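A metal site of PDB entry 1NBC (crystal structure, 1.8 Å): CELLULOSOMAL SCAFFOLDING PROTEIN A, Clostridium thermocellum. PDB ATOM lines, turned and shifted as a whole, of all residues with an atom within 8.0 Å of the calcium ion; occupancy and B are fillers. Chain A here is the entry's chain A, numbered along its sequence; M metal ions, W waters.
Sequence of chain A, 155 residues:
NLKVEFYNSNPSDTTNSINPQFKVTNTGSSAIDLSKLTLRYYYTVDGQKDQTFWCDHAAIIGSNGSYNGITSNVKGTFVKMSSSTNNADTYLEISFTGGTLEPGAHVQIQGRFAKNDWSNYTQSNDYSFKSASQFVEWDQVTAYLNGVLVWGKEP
O of Asp 46 lies within hydrogen-bond range of NZ of Lys 115, at 2.9 Å.
Of the 21 residues printed, 5 come within 4 Å of the calcium ion.
The calcium ion is bound by OD2 of Asp 46 (2.3 Å), O of Thr 122 (2.3 Å), OD1 of Asp 126 (2.4 Å), OG1 of Thr 44 (2.5 Å), O of Thr 44 (2.5 Å), OD1 of Asn 125 (2.6 Å) and water W1 (2.7 Å). The calcium ion has seven donor atoms within binding distance. Slightly farther from the calcium ion lies the side-chain carboxylate (OD1) of Asp 46 (2.9 Å).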
ATOM      1  N   ASP A  13      33.568  -2.928   1.459  1.00  0.00           N
ATOM      2  CA  ASP A  13      32.322  -3.288   2.108  1.00  0.00           C
ATOM      3  C   ASP A  13      31.725  -2.064   2.816  1.00  0.00           C
ATOM      4  O   ASP A  13      30.556  -1.725   2.622  1.00  0.00           O
ATOM      5  CB  ASP A  13      32.545  -4.466   3.086  1.00  0.00           C
ATOM      6  CG  ASP A  13      31.244  -4.998   3.663  1.00  0.00           C
ATOM      7  OD1 ASP A  13      30.224  -5.016   2.948  1.00  0.00           O
ATOM      8  OD2 ASP A  13      31.236  -5.382   4.845  1.00  0.00           O
ATOM      9  N   ILE A  18      29.367   4.908  -3.391  1.00  0.00           N
ATOM     10  CA  ILE A  18      29.146   3.715  -4.204  1.00  0.00           C
ATOM     11  C   ILE A  18      29.396   4.146  -5.655  1.00  0.00           C
ATOM     12  O   ILE A  18      28.918   5.198  -6.085  1.00  0.00           O
ATOM     13  CB  ILE A  18      27.715   3.147  -3.973  1.00  0.00           C
ATOM     14  CG1 ILE A  18      27.575   2.659  -2.530  1.00  0.00           C
ATOM     15  CG2 ILE A  18      27.440   2.002  -4.919  1.00  0.00           C
ATOM     16  CD1 ILE A  18      26.232   2.044  -2.208  1.00  0.00           C
ATOM     17  N   TYR A  42      19.881  -1.273  -7.487  1.00  0.00           N
ATOM     18  CA  TYR A  42      19.177  -1.531  -6.213  1.00  0.00           C
ATOM     19  C   TYR A  42      20.105  -1.823  -5.045  1.00  0.00           C
ATOM     20  O   TYR A  42      21.082  -2.571  -5.157  1.00  0.00           O
ATOM     21  CB  TYR A  42      18.216  -2.726  -6.360  1.00  0.00           C
ATOM     22  CG  TYR A  42      17.062  -2.530  -7.338  1.00  0.00           C
ATOM     23  CD1 TYR A  42      17.227  -2.802  -8.704  1.00  0.00           C
ATOM     24  CD2 TYR A  42      15.811  -2.081  -6.896  1.00  0.00           C
ATOM     25  CE1 TYR A  42      16.173  -2.642  -9.598  1.00  0.00           C
ATOM     26  CE2 TYR A  42      14.742  -1.922  -7.805  1.00  0.00           C
ATOM     27  CZ  TYR A  42      14.938  -2.202  -9.140  1.00  0.00           C
ATOM     28  OH  TYR A  42      13.907  -2.052 -10.037  1.00  0.00           O
ATOM     29  N   TYR A  43      19.778  -1.218  -3.897  1.00  0.00           N
ATOM     30  CA  TYR A  43      20.569  -1.375  -2.678  1.00  0.00           C
ATOM     31  C   TYR A  43      19.765  -1.016  -1.422  1.00  0.00           C
ATOM     32  O   TYR A  43      18.568  -0.747  -1.489  1.00  0.00           O
ATOM     33  CB  TYR A  43      21.806  -0.462  -2.738  1.00  0.00           C
ATOM     34  CG  TYR A  43      21.482   1.017  -2.812  1.00  0.00           C
ATOM     35  CD1 TYR A  43      20.972   1.594  -3.970  1.00  0.00           C
ATOM     36  CD2 TYR A  43      21.704   1.851  -1.697  1.00  0.00           C
ATOM     37  CE1 TYR A  43      20.683   2.965  -4.044  1.00  0.00           C
ATOM     38  CE2 TYR A  43      21.432   3.222  -1.755  1.00  0.00           C
ATOM     39  CZ  TYR A  43      20.924   3.779  -2.922  1.00  0.00           C
ATOM     40  OH  TYR A  43      20.650   5.120  -3.003  1.00  0.00           O
ATOM     41  N   THR A  44      20.429  -1.087  -0.275  1.00  0.00           N
ATOM     42  CA  THR A  44      19.849  -0.720   1.001  1.00  0.00           C
ATOM     43  C   THR A  44      20.625   0.499   1.457  1.00  0.00           C
ATOM     44  O   THR A  44      21.852   0.452   1.535  1.00  0.00           O
ATOM     45  CB  THR A  44      19.994  -1.851   2.018  1.00  0.00           C
ATOM     46  OG1 THR A  44      21.333  -2.335   1.993  1.00  0.00           O
ATOM     47  CG2 THR A  44      19.054  -2.965   1.700  1.00  0.00           C
ATOM     48  N   VAL A  45      19.929   1.607   1.702  1.00  0.00           N
ATOM     49  CA  VAL A  45      20.551   2.872   2.109  1.00  0.00           C
ATOM     50  C   VAL A  45      21.298   2.854   3.451  1.00  0.00           C
ATOM     51  O   VAL A  45      22.223   3.648   3.657  1.00  0.00           O
ATOM     52  CB  VAL A  45      19.518   4.007   2.057  1.00  0.00           C
ATOM     53  CG1 VAL A  45      18.539   3.889   3.223  1.00  0.00           C
ATOM     54  CG2 VAL A  45      20.206   5.351   2.023  1.00  0.00           C
ATOM     55  N   ASP A  46      20.968   1.897   4.326  1.00  0.00           N
ATOM     56  CA  ASP A  46      21.615   1.746   5.636  1.00  0.00           C
ATOM     57  C   ASP A  46      21.600   3.070   6.416  1.00  0.00           C
ATOM     58  O   ASP A  46      22.636   3.548   6.866  1.00  0.00           O
ATOM     59  CB  ASP A  46      23.069   1.265   5.480  1.00  0.00           C
ATOM     60  CG  ASP A  46      23.194   0.073   4.536  1.00  0.00           C
ATOM     61  OD1 ASP A  46      22.356  -0.846   4.598  1.00  0.00           O
ATOM     62  OD2 ASP A  46      24.140   0.072   3.716  1.00  0.00           O
ATOM     63  N   GLY A  47      20.405   3.590   6.645  1.00  0.00           N
ATOM     64  CA  GLY A  47      20.277   4.860   7.325  1.00  0.00           C
ATOM     65  C   GLY A  47      19.882   5.872   6.281  1.00  0.00           C
ATOM     66  O   GLY A  47      20.707   6.276   5.466  1.00  0.00           O
ATOM     67  N   ASN A  86      15.191  -7.571   1.778  1.00  0.00           N
ATOM     68  CA  ASN A  86      16.290  -7.448   2.730  1.00  0.00           C
ATOM     69  C   ASN A  86      17.613  -6.925   2.149  1.00  0.00           C
ATOM     70  O   ASN A  86      18.547  -6.609   2.902  1.00  0.00           O
ATOM     71  CB  ASN A  86      16.470  -8.738   3.557  1.00  0.00           C
ATOM     72  CG  ASN A  86      17.414  -9.730   2.919  1.00  0.00           C
ATOM     73  OD1 ASN A  86      17.059 -10.407   1.940  1.00  0.00           O
ATOM     74  ND2 ASN A  86      18.617  -9.835   3.472  1.00  0.00           N
ATOM     75  N   ASN A  87      17.722  -6.858   0.819  1.00  0.00           N
ATOM     76  CA  ASN A  87      18.924  -6.310   0.220  1.00  0.00           C
ATOM     77  C   ASN A  87      18.588  -5.246  -0.816  1.00  0.00           C
ATOM     78  O   ASN A  87      19.430  -4.901  -1.646  1.00  0.00           O
ATOM     79  CB  ASN A  87      19.844  -7.401  -0.331  1.00  0.00           C
ATOM     80  CG  ASN A  87      19.215  -8.159  -1.461  1.00  0.00           C
ATOM     81  OD1 ASN A  87      18.008  -8.092  -1.669  1.00  0.00           O
ATOM     82  ND2 ASN A  87      20.033  -8.905  -2.191  1.00  0.00           N
ATOM     83  N   ALA A  88      17.371  -4.707  -0.751  1.00  0.00           N
ATOM     84  CA  ALA A  88      16.960  -3.635  -1.654  1.00  0.00           C
ATOM     85  C   ALA A  88      15.783  -2.832  -1.092  1.00  0.00           C
ATOM     86  O   ALA A  88      14.679  -3.340  -0.966  1.00  0.00           O
ATOM     87  CB  ALA A  88      16.608  -4.175  -3.019  1.00  0.00           C
ATOM     88  N   ASP A  89      16.042  -1.581  -0.728  1.00  0.00           N
ATOM     89  CA  ASP A  89      14.970  -0.704  -0.237  1.00  0.00           C
ATOM     90  C   ASP A  89      14.989   0.643  -0.937  1.00  0.00           C
ATOM     91  O   ASP A  89      14.084   1.434  -0.792  1.00  0.00           O
ATOM     92  CB  ASP A  89      14.998  -0.535   1.295  1.00  0.00           C
ATOM     93  CG  ASP A  89      16.279   0.102   1.815  1.00  0.00           C
ATOM     94  OD1 ASP A  89      16.966   0.872   1.095  1.00  0.00           O
ATOM     95  OD2 ASP A  89      16.592  -0.142   2.996  1.00  0.00           O
ATOM     96  N   LYS A 115      25.835   9.899   0.442  1.00  0.00           N
ATOM     97  CA  LYS A 115      24.883  10.541   1.337  1.00  0.00           C
ATOM     98  C   LYS A 115      25.375  11.970   1.545  1.00  0.00           C
ATOM     99  O   LYS A 115      26.579  12.222   1.597  1.00  0.00           O
ATOM    100  CB  LYS A 115      24.820   9.795   2.667  1.00  0.00           C
ATOM    101  CG  LYS A 115      24.200   8.443   2.555  1.00  0.00           C
ATOM    102  CD  LYS A 115      24.404   7.626   3.813  1.00  0.00           C
ATOM    103  CE  LYS A 115      23.580   6.366   3.741  1.00  0.00           C
ATOM    104  NZ  LYS A 115      23.677   5.515   4.943  1.00  0.00           N
ATOM    105  N   ASN A 120      28.541   6.349   6.098  1.00  0.00           N
ATOM    106  CA  ASN A 120      28.816   5.094   5.412  1.00  0.00           C
ATOM    107  C   ASN A 120      27.630   4.280   4.943  1.00  0.00           C
ATOM    108  O   ASN A 120      26.531   4.385   5.474  1.00  0.00           O
ATOM    109  CB  ASN A 120      29.677   4.177   6.271  1.00  0.00           C
ATOM    110  CG  ASN A 120      31.102   4.668   6.426  1.00  0.00           C
ATOM    111  OD1 ASN A 120      31.740   5.105   5.468  1.00  0.00           O
ATOM    112  ND2 ASN A 120      31.632   4.562   7.635  1.00  0.00           N
ATOM    113  N   TYR A 121      27.906   3.454   3.945  1.00  0.00           N
ATOM    114  CA  TYR A 121      26.990   2.499   3.373  1.00  0.00           C
ATOM    115  C   TYR A 121      27.631   1.162   3.654  1.00  0.00           C
ATOM    116  O   TYR A 121      28.820   1.094   3.951  1.00  0.00           O
ATOM    117  CB  TYR A 121      26.906   2.579   1.855  1.00  0.00           C
ATOM    118  CG  TYR A 121      26.285   3.785   1.233  1.00  0.00           C
ATOM    119  CD1 TYR A 121      24.932   3.857   1.020  1.00  0.00           C
ATOM    120  CD2 TYR A 121      27.069   4.850   0.797  1.00  0.00           C
ATOM    121  CE1 TYR A 121      24.362   4.945   0.381  1.00  0.00           C
ATOM    122  CE2 TYR A 121      26.508   5.948   0.162  1.00  0.00           C
ATOM    123  CZ  TYR A 121      25.154   5.981  -0.041  1.00  0.00           C
ATOM    124  OH  TYR A 121      24.581   7.038  -0.702  1.00  0.00           O
ATOM    125  N   THR A 122      26.865   0.104   3.508  1.00  0.00           N
ATOM    126  CA  THR A 122      27.377  -1.238   3.633  1.00  0.00           C
ATOM    127  C   THR A 122      26.985  -1.879   2.306  1.00  0.00           C
ATOM    128  O   THR A 122      25.798  -1.902   1.946  1.00  0.00           O
ATOM    129  CB  THR A 122      26.733  -1.995   4.808  1.00  0.00           C
ATOM    130  OG1 THR A 122      27.157  -1.394   6.039  1.00  0.00           O
ATOM    131  CG2 THR A 122      27.188  -3.440   4.798  1.00  0.00           C
ATOM    132  N   GLN A 123      27.972  -2.309   1.538  1.00  0.00           N
ATOM    133  CA  GLN A 123      27.720  -2.865   0.225  1.00  0.00           C
ATOM    134  C   GLN A 123      27.401  -4.367   0.177  1.00  0.00           C
ATOM    135  O   GLN A 123      26.892  -4.830  -0.839  1.00  0.00           O
ATOM    136  CB  GLN A 123      28.875  -2.540  -0.726  1.00  0.00           C
ATOM    137  CG  GLN A 123      29.164  -1.050  -0.876  1.00  0.00           C
ATOM    138  CD  GLN A 123      29.885  -0.742  -2.176  1.00  0.00           C
ATOM    139  OE1 GLN A 123      29.252  -0.539  -3.208  1.00  0.00           O
ATOM    140  NE2 GLN A 123      31.198  -0.737  -2.144  1.00  0.00           N
ATOM    141  N   SER A 124      27.656  -5.093   1.263  1.00  0.00           N
ATOM    142  CA  SER A 124      27.406  -6.543   1.290  1.00  0.00           C
ATOM    143  C   SER A 124      25.930  -6.923   1.381  1.00  0.00           C
ATOM    144  O   SER A 124      25.615  -8.105   1.315  1.00  0.00           O
ATOM    145  CB  SER A 124      28.177  -7.241   2.404  1.00  0.00           C
ATOM    146  OG  SER A 124      27.952  -6.622   3.659  1.00  0.00           O
ATOM    147  N   ASN A 125      25.047  -5.952   1.598  1.00  0.00           N
ATOM    148  CA  ASN A 125      23.621  -6.221   1.653  1.00  0.00           C
ATOM    149  C   ASN A 125      22.869  -5.422   0.566  1.00  0.00           C
ATOM    150  O   ASN A 125      21.704  -5.081   0.720  1.00  0.00           O
ATOM    151  CB  ASN A 125      23.052  -5.953   3.069  1.00  0.00           C
ATOM    152  CG  ASN A 125      23.271  -4.542   3.536  1.00  0.00           C
ATOM    153  OD1 ASN A 125      23.884  -3.724   2.845  1.00  0.00           O
ATOM    154  ND2 ASN A 125      22.746  -4.224   4.713  1.00  0.00           N
ATOM    155  N   ASP A 126      23.566  -5.183  -0.553  1.00  0.00           N
ATOM    156  CA  ASP A 126      23.050  -4.467  -1.712  1.00  0.00           C
ATOM    157  C   ASP A 126      22.825  -5.401  -2.871  1.00  0.00           C
ATOM    158  O   ASP A 126      23.783  -5.991  -3.397  1.00  0.00           O
ATOM    159  CB  ASP A 126      24.037  -3.404  -2.156  1.00  0.00           C
ATOM    160  CG  ASP A 126      24.165  -2.294  -1.173  1.00  0.00           C
ATOM    161  OD1 ASP A 126      23.335  -2.228  -0.231  1.00  0.00           O
ATOM    162  OD2 ASP A 126      25.094  -1.483  -1.343  1.00  0.00           O
ATOM    163  N   TYR A 127      21.581  -5.436  -3.344  1.00  0.00           N
ATOM    164  CA  TYR A 127      21.152  -6.297  -4.432  1.00  0.00           C
ATOM    165  C   TYR A 127      21.969  -6.205  -5.713  1.00  0.00           C
ATOM    166  O   TYR A 127      22.336  -7.226  -6.284  1.00  0.00           O
ATOM    167  CB  TYR A 127      19.685  -5.999  -4.774  1.00  0.00           C
ATOM    168  CG  TYR A 127      19.114  -6.865  -5.876  1.00  0.00           C
ATOM    169  CD1 TYR A 127      18.725  -8.198  -5.630  1.00  0.00           C
ATOM    170  CD2 TYR A 127      18.945  -6.367  -7.177  1.00  0.00           C
ATOM    171  CE1 TYR A 127      18.188  -9.002  -6.647  1.00  0.00           C
ATOM    172  CE2 TYR A 127      18.400  -7.151  -8.207  1.00  0.00           C
ATOM    173  CZ  TYR A 127      18.025  -8.474  -7.936  1.00  0.00           C
ATOM    174  OH  TYR A 127      17.502  -9.257  -8.937  1.00  0.00           O
HETATM  175 CA    CA M   1      23.577  -1.318   1.993  1.00  0.00          CA
HETATM  176  O   HOH W   1      24.926   0.473   0.567  1.00  0.00           O
